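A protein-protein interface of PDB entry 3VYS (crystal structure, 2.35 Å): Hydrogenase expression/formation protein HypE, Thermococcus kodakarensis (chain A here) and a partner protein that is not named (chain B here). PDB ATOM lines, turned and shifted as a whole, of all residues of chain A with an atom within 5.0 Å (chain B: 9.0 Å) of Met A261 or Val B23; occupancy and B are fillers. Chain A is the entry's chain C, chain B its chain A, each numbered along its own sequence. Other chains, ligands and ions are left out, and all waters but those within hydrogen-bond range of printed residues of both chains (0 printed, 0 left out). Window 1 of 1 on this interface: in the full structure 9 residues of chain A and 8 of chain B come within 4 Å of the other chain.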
ATOM      1  N   ILE A 187      -9.752 -14.905   5.674  1.00  0.00           N
ATOM      2  CA  ILE A 187      -9.261 -14.216   4.486  1.00  0.00           C
ATOM      3  C   ILE A 187      -7.749 -13.992   4.548  1.00  0.00           C
ATOM      4  O   ILE A 187      -7.257 -13.335   5.468  1.00  0.00           O
ATOM      5  CB  ILE A 187      -9.988 -12.872   4.329  1.00  0.00           C
ATOM      6  CG1 ILE A 187     -11.471 -13.137   4.025  1.00  0.00           C
ATOM      7  CG2 ILE A 187      -9.336 -12.053   3.245  1.00  0.00           C
ATOM      8  CD1 ILE A 187     -12.291 -11.876   3.913  1.00  0.00           C
ATOM      9  N   ALA A 188      -7.025 -14.533   3.564  1.00  0.00           N
ATOM     10  CA  ALA A 188      -5.561 -14.428   3.498  1.00  0.00           C
ATOM     11  C   ALA A 188      -5.052 -13.174   2.768  1.00  0.00           C
ATOM     12  O   ALA A 188      -5.831 -12.326   2.374  1.00  0.00           O
ATOM     13  CB  ALA A 188      -4.988 -15.689   2.845  1.00  0.00           C
ATOM     14  N   PHE A 189      -3.740 -13.064   2.597  1.00  0.00           N
ATOM     15  CA  PHE A 189      -3.184 -11.890   1.933  1.00  0.00           C
ATOM     16  C   PHE A 189      -1.830 -12.075   1.249  1.00  0.00           C
ATOM     17  O   PHE A 189      -1.137 -13.067   1.446  1.00  0.00           O
ATOM     18  CB  PHE A 189      -3.107 -10.738   2.929  1.00  0.00           C
ATOM     19  CG  PHE A 189      -4.386 -10.500   3.648  1.00  0.00           C
ATOM     20  CD1 PHE A 189      -5.429  -9.836   3.034  1.00  0.00           C
ATOM     21  CD2 PHE A 189      -4.557 -10.972   4.936  1.00  0.00           C
ATOM     22  CE1 PHE A 189      -6.614  -9.627   3.700  1.00  0.00           C
ATOM     23  CE2 PHE A 189      -5.742 -10.766   5.608  1.00  0.00           C
ATOM     24  CZ  PHE A 189      -6.773 -10.092   4.989  1.00  0.00           C
ATOM     25  N   GLU A 254      -5.799  -2.882   0.982  1.00  0.00           N
ATOM     26  CA  GLU A 254      -6.206  -4.124   1.627  1.00  0.00           C
ATOM     27  C   GLU A 254      -7.461  -3.886   2.453  1.00  0.00           C
ATOM     28  O   GLU A 254      -8.356  -4.728   2.491  1.00  0.00           O
ATOM     29  CB  GLU A 254      -5.096  -4.659   2.551  1.00  0.00           C
ATOM     30  CG  GLU A 254      -3.692  -4.608   1.978  1.00  0.00           C
ATOM     31  CD  GLU A 254      -2.992  -3.288   2.267  1.00  0.00           C
ATOM     32  OE1 GLU A 254      -2.314  -3.183   3.315  1.00  0.00           O
ATOM     33  OE2 GLU A 254      -3.132  -2.349   1.456  1.00  0.00           O
ATOM     34  N   ALA A 257     -10.545  -3.228   0.029  1.00  0.00           N
ATOM     35  CA  ALA A 257     -10.900  -4.531  -0.514  1.00  0.00           C
ATOM     36  C   ALA A 257     -11.622  -5.428   0.486  1.00  0.00           C
ATOM     37  O   ALA A 257     -12.707  -5.942   0.203  1.00  0.00           O
ATOM     38  CB  ALA A 257      -9.649  -5.219  -1.023  1.00  0.00           C
ATOM     39  N   ALA A 258     -11.025  -5.608   1.659  1.00  0.00           N
ATOM     40  CA  ALA A 258     -11.618  -6.454   2.687  1.00  0.00           C
ATOM     41  C   ALA A 258     -12.933  -5.900   3.225  1.00  0.00           C
ATOM     42  O   ALA A 258     -13.870  -6.661   3.486  1.00  0.00           O
ATOM     43  CB  ALA A 258     -10.628  -6.656   3.838  1.00  0.00           C
ATOM     44  N   SER A 259     -13.005  -4.581   3.402  1.00  0.00           N
ATOM     45  CA  SER A 259     -14.226  -3.966   3.922  1.00  0.00           C
ATOM     46  C   SER A 259     -15.362  -4.230   2.945  1.00  0.00           C
ATOM     47  O   SER A 259     -16.475  -4.568   3.347  1.00  0.00           O
ATOM     48  CB  SER A 259     -14.043  -2.454   4.118  1.00  0.00           C
ATOM     49  OG  SER A 259     -14.070  -1.759   2.883  1.00  0.00           O
ATOM     50  N   GLU A 260     -15.072  -4.082   1.657  1.00  0.00           N
ATOM     51  CA  GLU A 260     -16.072  -4.324   0.630  1.00  0.00           C
ATOM     52  C   GLU A 260     -16.601  -5.740   0.737  1.00  0.00           C
ATOM     53  O   GLU A 260     -17.804  -5.948   0.867  1.00  0.00           O
ATOM     54  CB  GLU A 260     -15.481  -4.090  -0.758  1.00  0.00           C
ATOM     55  CG  GLU A 260     -15.506  -2.635  -1.174  1.00  0.00           C
ATOM     56  CD  GLU A 260     -16.918  -2.077  -1.187  1.00  0.00           C
ATOM     57  OE1 GLU A 260     -17.745  -2.574  -1.982  1.00  0.00           O
ATOM     58  OE2 GLU A 260     -17.204  -1.149  -0.398  1.00  0.00           O
ATOM     59  N   MET A 261     -15.702  -6.716   0.690  1.00  0.00           N
ATOM     60  CA  MET A 261     -16.105  -8.111   0.792  1.00  0.00           C
ATOM     61  C   MET A 261     -16.853  -8.372   2.094  1.00  0.00           C
ATOM     62  O   MET A 261     -17.790  -9.170   2.135  1.00  0.00           O
ATOM     63  CB  MET A 261     -14.882  -9.019   0.708  1.00  0.00           C
ATOM     64  CG  MET A 261     -14.272  -9.080  -0.672  1.00  0.00           C
ATOM     65  SD  MET A 261     -12.794 -10.086  -0.691  1.00  0.00           S
ATOM     66  CE  MET A 261     -11.548  -8.827  -0.772  1.00  0.00           C
ATOM     67  N   LEU A 262     -16.436  -7.696   3.159  1.00  0.00           N
ATOM     68  CA  LEU A 262     -17.079  -7.862   4.452  1.00  0.00           C
ATOM     69  C   LEU A 262     -18.379  -7.067   4.513  1.00  0.00           C
ATOM     70  O   LEU A 262     -19.228  -7.310   5.369  1.00  0.00           O
ATOM     71  CB  LEU A 262     -16.127  -7.416   5.563  1.00  0.00           C
ATOM     72  CG  LEU A 262     -14.875  -8.284   5.728  1.00  0.00           C
ATOM     73  CD1 LEU A 262     -13.944  -7.674   6.761  1.00  0.00           C
ATOM     74  CD2 LEU A 262     -15.282  -9.687   6.149  1.00  0.00           C
ATOM     75  N   GLY A 263     -18.530  -6.119   3.593  1.00  0.00           N
ATOM     76  CA  GLY A 263     -19.729  -5.300   3.556  1.00  0.00           C
ATOM     77  C   GLY A 263     -19.828  -4.328   4.719  1.00  0.00           C
ATOM     78  O   GLY A 263     -20.920  -4.040   5.207  1.00  0.00           O
ATOM     79  N   CYS B   1     -25.103  -9.600  -3.429  1.00  0.00           N
ATOM     80  CA  CYS B   1     -24.509  -9.128  -4.720  1.00  0.00           C
ATOM     81  C   CYS B   1     -23.507  -8.006  -4.471  1.00  0.00           C
ATOM     82  O   CYS B   1     -23.653  -6.892  -4.982  1.00  0.00           O
ATOM     83  CB  CYS B   1     -25.620  -8.648  -5.667  1.00  0.00           C
ATOM     84  SG  CYS B   1     -25.099  -8.288  -7.375  1.00  0.00           S
ATOM     85  N   LEU B   2     -22.491  -8.300  -3.670  1.00  0.00           N
ATOM     86  CA  LEU B   2     -21.468  -7.303  -3.392  1.00  0.00           C
ATOM     87  C   LEU B   2     -20.739  -7.023  -4.700  1.00  0.00           C
ATOM     88  O   LEU B   2     -20.335  -5.896  -4.981  1.00  0.00           O
ATOM     89  CB  LEU B   2     -20.501  -7.820  -2.325  1.00  0.00           C
ATOM     90  CG  LEU B   2     -21.190  -8.234  -1.014  1.00  0.00           C
ATOM     91  CD1 LEU B   2     -20.203  -8.178   0.137  1.00  0.00           C
ATOM     92  CD2 LEU B   2     -22.350  -7.296  -0.743  1.00  0.00           C
ATOM     93  N   ALA B   3     -20.576  -8.071  -5.495  1.00  0.00           N
ATOM     94  CA  ALA B   3     -19.948  -7.960  -6.800  1.00  0.00           C
ATOM     95  C   ALA B   3     -18.656  -7.162  -6.881  1.00  0.00           C
ATOM     96  O   ALA B   3     -18.603  -6.122  -7.543  1.00  0.00           O
ATOM     97  CB  ALA B   3     -20.936  -7.379  -7.757  1.00  0.00           C
ATOM     98  N   VAL B   4     -17.610  -7.652  -6.235  1.00  0.00           N
ATOM     99  CA  VAL B   4     -16.329  -6.969  -6.287  1.00  0.00           C
ATOM    100  C   VAL B   4     -15.486  -7.690  -7.347  1.00  0.00           C
ATOM    101  O   VAL B   4     -15.539  -8.914  -7.472  1.00  0.00           O
ATOM    102  CB  VAL B   4     -15.639  -6.957  -4.864  1.00  0.00           C
ATOM    103  CG1 VAL B   4     -15.571  -8.362  -4.305  1.00  0.00           C
ATOM    104  CG2 VAL B   4     -14.241  -6.320  -4.936  1.00  0.00           C
ATOM    105  N   PRO B   5     -14.750  -6.923  -8.169  1.00  0.00           N
ATOM    106  CA  PRO B   5     -13.897  -7.484  -9.224  1.00  0.00           C
ATOM    107  C   PRO B   5     -12.517  -7.879  -8.712  1.00  0.00           C
ATOM    108  O   PRO B   5     -11.963  -7.237  -7.825  1.00  0.00           O
ATOM    109  CB  PRO B   5     -13.800  -6.350 -10.242  1.00  0.00           C
ATOM    110  CG  PRO B   5     -14.971  -5.461  -9.915  1.00  0.00           C
ATOM    111  CD  PRO B   5     -14.991  -5.495  -8.419  1.00  0.00           C
ATOM    112  N   GLY B   6     -11.959  -8.929  -9.300  1.00  0.00           N
ATOM    113  CA  GLY B   6     -10.642  -9.387  -8.901  1.00  0.00           C
ATOM    114  C   GLY B   6      -9.845  -9.941 -10.064  1.00  0.00           C
ATOM    115  O   GLY B   6     -10.408 -10.300 -11.099  1.00  0.00           O
ATOM    116  N   LYS B   7      -8.529 -10.005  -9.893  1.00  0.00           N
ATOM    117  CA  LYS B   7      -7.663 -10.517 -10.933  1.00  0.00           C
ATOM    118  C   LYS B   7      -7.294 -11.953 -10.623  1.00  0.00           C
ATOM    119  O   LYS B   7      -6.673 -12.242  -9.600  1.00  0.00           O
ATOM    120  CB  LYS B   7      -6.393  -9.672 -11.047  1.00  0.00           C
ATOM    121  CG  LYS B   7      -5.554  -9.999 -12.278  1.00  0.00           C
ATOM    122  CD  LYS B   7      -4.287  -9.153 -12.353  1.00  0.00           C
ATOM    123  CE  LYS B   7      -3.245  -9.586 -11.322  1.00  0.00           C
ATOM    124  NZ  LYS B   7      -3.714  -9.490  -9.907  1.00  0.00           N
ATOM    125  N   ILE B   9      -5.319 -15.139 -10.459  1.00  0.00           N
ATOM    126  CA  ILE B   9      -3.881 -15.363 -10.456  1.00  0.00           C
ATOM    127  C   ILE B   9      -3.519 -16.848 -10.529  1.00  0.00           C
ATOM    128  O   ILE B   9      -2.354 -17.198 -10.707  1.00  0.00           O
ATOM    129  CB  ILE B   9      -3.218 -14.748  -9.202  1.00  0.00           C
ATOM    130  CG1 ILE B   9      -3.680 -15.484  -7.942  1.00  0.00           C
ATOM    131  CG2 ILE B   9      -3.563 -13.268  -9.113  1.00  0.00           C
ATOM    132  CD1 ILE B   9      -2.961 -15.046  -6.676  1.00  0.00           C
ATOM    133  N   VAL B  17      -7.804 -18.698  -7.863  1.00  0.00           N
ATOM    134  CA  VAL B  17      -7.392 -17.822  -6.775  1.00  0.00           C
ATOM    135  C   VAL B  17      -7.470 -16.396  -7.302  1.00  0.00           C
ATOM    136  O   VAL B  17      -6.638 -15.967  -8.105  1.00  0.00           O
ATOM    137  CB  VAL B  17      -5.955 -18.117  -6.321  1.00  0.00           C
ATOM    138  CG1 VAL B  17      -5.576 -17.198  -5.176  1.00  0.00           C
ATOM    139  CG2 VAL B  17      -5.834 -19.568  -5.904  1.00  0.00           C
ATOM    140  N   VAL B  18      -8.484 -15.670  -6.847  1.00  0.00           N
ATOM    141  CA  VAL B  18      -8.711 -14.302  -7.277  1.00  0.00           C
ATOM    142  C   VAL B  18      -8.121 -13.295  -6.300  1.00  0.00           C
ATOM    143  O   VAL B  18      -8.195 -13.472  -5.084  1.00  0.00           O
ATOM    144  CB  VAL B  18     -10.222 -14.053  -7.449  1.00  0.00           C
ATOM    145  CG1 VAL B  18     -10.477 -12.640  -7.949  1.00  0.00           C
ATOM    146  CG2 VAL B  18     -10.798 -15.079  -8.417  1.00  0.00           C
ATOM    147  N   ASP B  19      -7.528 -12.236  -6.843  1.00  0.00           N
ATOM    148  CA  ASP B  19      -6.917 -11.198  -6.019  1.00  0.00           C
ATOM    149  C   ASP B  19      -7.735  -9.910  -6.061  1.00  0.00           C
ATOM    150  O   ASP B  19      -7.885  -9.288  -7.115  1.00  0.00           O
ATOM    151  CB  ASP B  19      -5.489 -10.908  -6.498  1.00  0.00           C
ATOM    152  CG  ASP B  19      -4.791  -9.844  -5.656  1.00  0.00           C
ATOM    153  OD1 ASP B  19      -3.642  -9.481  -5.990  1.00  0.00           O
ATOM    154  OD2 ASP B  19      -5.385  -9.370  -4.661  1.00  0.00           O
ATOM    155  N   PHE B  20      -8.255  -9.516  -4.905  1.00  0.00           N
ATOM    156  CA  PHE B  20      -9.043  -8.306  -4.807  1.00  0.00           C
ATOM    157  C   PHE B  20      -8.220  -7.217  -4.147  1.00  0.00           C
ATOM    158  O   PHE B  20      -8.492  -6.804  -3.026  1.00  0.00           O
ATOM    159  CB  PHE B  20     -10.313  -8.559  -4.003  1.00  0.00           C
ATOM    160  CG  PHE B  20     -11.220  -9.581  -4.613  1.00  0.00           C
ATOM    161  CD1 PHE B  20     -11.067 -10.931  -4.335  1.00  0.00           C
ATOM    162  CD2 PHE B  20     -12.223  -9.194  -5.487  1.00  0.00           C
ATOM    163  CE1 PHE B  20     -11.905 -11.882  -4.924  1.00  0.00           C
ATOM    164  CE2 PHE B  20     -13.060 -10.137  -6.079  1.00  0.00           C
ATOM    165  CZ  PHE B  20     -12.902 -11.484  -5.797  1.00  0.00           C
ATOM    166  N   GLY B  21      -7.186  -6.773  -4.846  1.00  0.00           N
ATOM    167  CA  GLY B  21      -6.335  -5.725  -4.321  1.00  0.00           C
ATOM    168  C   GLY B  21      -5.683  -6.105  -3.003  1.00  0.00           C
ATOM    169  O   GLY B  21      -6.007  -5.541  -1.959  1.00  0.00           O
ATOM    170  N   GLY B  22      -4.765  -7.067  -3.042  1.00  0.00           N
ATOM    171  CA  GLY B  22      -4.063  -7.472  -1.835  1.00  0.00           C
ATOM    172  C   GLY B  22      -4.810  -8.405  -0.907  1.00  0.00           C
ATOM    173  O   GLY B  22      -4.419  -8.594   0.246  1.00  0.00           O
ATOM    174  N   VAL B  23      -5.890  -8.985  -1.411  1.00  0.00           N
ATOM    175  CA  VAL B  23      -6.701  -9.923  -0.642  1.00  0.00           C
ATOM    176  C   VAL B  23      -7.122 -11.040  -1.589  1.00  0.00           C
ATOM    177  O   VAL B  23      -7.826 -10.800  -2.566  1.00  0.00           O
ATOM    178  CB  VAL B  23      -7.963  -9.244  -0.090  1.00  0.00           C
ATOM    179  CG1 VAL B  23      -8.876 -10.273   0.553  1.00  0.00           C
ATOM    180  CG2 VAL B  23      -7.572  -8.167   0.919  1.00  0.00           C
ATOM    181  N   LYS B  24      -6.698 -12.262  -1.299  1.00  0.00           N
ATOM    182  CA  LYS B  24      -7.022 -13.385  -2.167  1.00  0.00           C
ATOM    183  C   LYS B  24      -8.073 -14.308  -1.581  1.00  0.00           C
ATOM    184  O   LYS B  24      -8.163 -14.466  -0.366  1.00  0.00           O
ATOM    185  CB  LYS B  24      -5.748 -14.180  -2.475  1.00  0.00           C
ATOM    186  CG  LYS B  24      -4.604 -13.323  -3.001  1.00  0.00           C
ATOM    187  CD  LYS B  24      -3.331 -14.133  -3.195  1.00  0.00           C
ATOM    188  CE  LYS B  24      -2.204 -13.266  -3.734  1.00  0.00           C
ATOM    189  NZ  LYS B  24      -0.978 -14.067  -3.997  1.00  0.00           N
ATOM    190  N   ARG B  25      -8.868 -14.904  -2.469  1.00  0.00           N
ATOM    191  CA  ARG B  25      -9.923 -15.842  -2.094  1.00  0.00           C
ATOM    192  C   ARG B  25     -10.084 -16.840  -3.234  1.00  0.00           C
ATOM    193  O   ARG B  25      -9.833 -16.501  -4.391  1.00  0.00           O
ATOM    194  CB  ARG B  25     -11.263 -15.126  -1.895  1.00  0.00           C
ATOM    195  CG  ARG B  25     -11.201 -13.851  -1.077  1.00  0.00           C
ATOM    196  CD  ARG B  25     -12.557 -13.493  -0.470  1.00  0.00           C
ATOM    197  NE  ARG B  25     -12.870 -14.317   0.698  1.00  0.00           N
ATOM    198  CZ  ARG B  25     -13.390 -15.540   0.651  1.00  0.00           C
ATOM    199  NH1 ARG B  25     -13.677 -16.107  -0.514  1.00  0.00           N
ATOM    200  NH2 ARG B  25     -13.609 -16.207   1.777  1.00  0.00           N
ATOM    201  N   GLU B  26     -10.503 -18.062  -2.914  1.00  0.00           N
ATOM    202  CA  GLU B  26     -10.710 -19.083  -3.936  1.00  0.00           C
ATOM    203  C   GLU B  26     -12.102 -18.932  -4.536  1.00  0.00           C
ATOM    204  O   GLU B  26     -13.068 -18.698  -3.821  1.00  0.00           O
ATOM    205  CB  GLU B  26     -10.534 -20.483  -3.342  1.00  0.00           C
ATOM    206  CG  GLU B  26      -9.080 -20.868  -3.112  1.00  0.00           C
ATOM    207  CD  GLU B  26      -8.906 -22.320  -2.705  1.00  0.00           C
ATOM    208  OE1 GLU B  26      -9.433 -23.210  -3.408  1.00  0.00           O
ATOM    209  OE2 GLU B  26      -8.234 -22.571  -1.684  1.00  0.00           O
ATOM    210  N   VAL B  27     -12.197 -19.075  -5.852  1.00  0.00           N
ATOM    211  CA  VAL B  27     -13.465 -18.915  -6.550  1.00  0.00           C
ATOM    212  C   VAL B  27     -13.775 -20.052  -7.514  1.00  0.00           C
ATOM    213  O   VAL B  27     -12.894 -20.527  -8.224  1.00  0.00           O
ATOM    214  CB  VAL B  27     -13.462 -17.603  -7.360  1.00  0.00           C
ATOM    215  CG1 VAL B  27     -14.804 -17.398  -8.025  1.00  0.00           C
ATOM    216  CG2 VAL B  27     -13.112 -16.434  -6.452  1.00  0.00           C
ATOM    217  N   VAL B  43     -17.109 -11.554  -8.933  1.00  0.00           N
ATOM    218  CA  VAL B  43     -17.387 -12.689  -8.071  1.00  0.00           C
ATOM    219  C   VAL B  43     -18.618 -12.488  -7.202  1.00  0.00           C
ATOM    220  O   VAL B  43     -18.694 -11.532  -6.426  1.00  0.00           O
ATOM    221  CB  VAL B  43     -16.173 -12.995  -7.168  1.00  0.00           C
ATOM    222  CG1 VAL B  43     -16.400 -14.290  -6.411  1.00  0.00           C
ATOM    223  CG2 VAL B  43     -14.911 -13.068  -8.017  1.00  0.00           C
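O of Val B4 sits at hydrogen-bond distance from N of Val B43 (3.4 Å).
The backbone NH (N) of Gly B22 is in hydrogen-bond range of the side-chain carboxylate (OD2) of Asp B19 (2.9 Å).
N of Val B23 is in hydrogen-bond range of OD2 of Asp B19 (3.3 Å).
O of Arg B25 lies within hydrogen-bond range of N of Val B18 (2.9 Å).
The side-chain carboxylate (OD2) of Asp B19 sits at hydrogen-bond distance from the backbone NH (N) of Gly B21, at 3.2 Å.
Val B23 touches Ile A187 (CG1 to CG2, 3.3 Å).
O of Ala A188 touches N of Lys B24, 3.8 Å away.
Val B23 touches Phe A189 (CG2 to CE1, 3.3 Å).
Ala A257 touches Phe B20 (CB to O, 2.8 Å).
CB of Ala A257 touches O of Gly B21, at 3.8 Å.
O of Glu A260 touches CD1 of Leu B2, 3.4 Å away.
CD1 of Leu B2 touches O of Met A261 (3.3 Å).
Val B4 touches Met A261 (CG1 to CG, 3.9 Å).
CE of Met A261 touches CB of Phe B20, at 3.5 Å.
Val B23 touches Met A261 (CG1 to CE, 3.3 Å).
Met A261 touches just these residues of chain B: Leu B2 (3.3 Å), Val B4 (3.9 Å), Phe B20 (3.5 Å), Val B23 (3.3 Å) and Arg B25 (3.4 Å).
Val B23 touches five residues of chain A.
Of the printed residues of chain B, Ala A188 touches Val B23 and Lys B24.
Printed residues of chain A within 4 Å of Val B4: Met A261 (3.9 Å).
Printed residues of chain B within 4 Å of Glu A254: Gly B21 and Val B23.
Hydrophobic or aromatic side chains of chain A within 4 Å of the printed part of chain B: Ile A187, Phe A189, Ala A257 and Met A261.
Of the 20 printed residues of chain B, 8 touch a printed residue of chain A.
Hydrophobic or aromatic side chains of chain B that line the printed part of chain A: Leu B2, Val B4, Phe B20 and Val B23.
Among the printed residues, no Asp or Glu carboxylate lies within 4 Å of a Lys or Arg side-chain nitrogen of the other chain.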
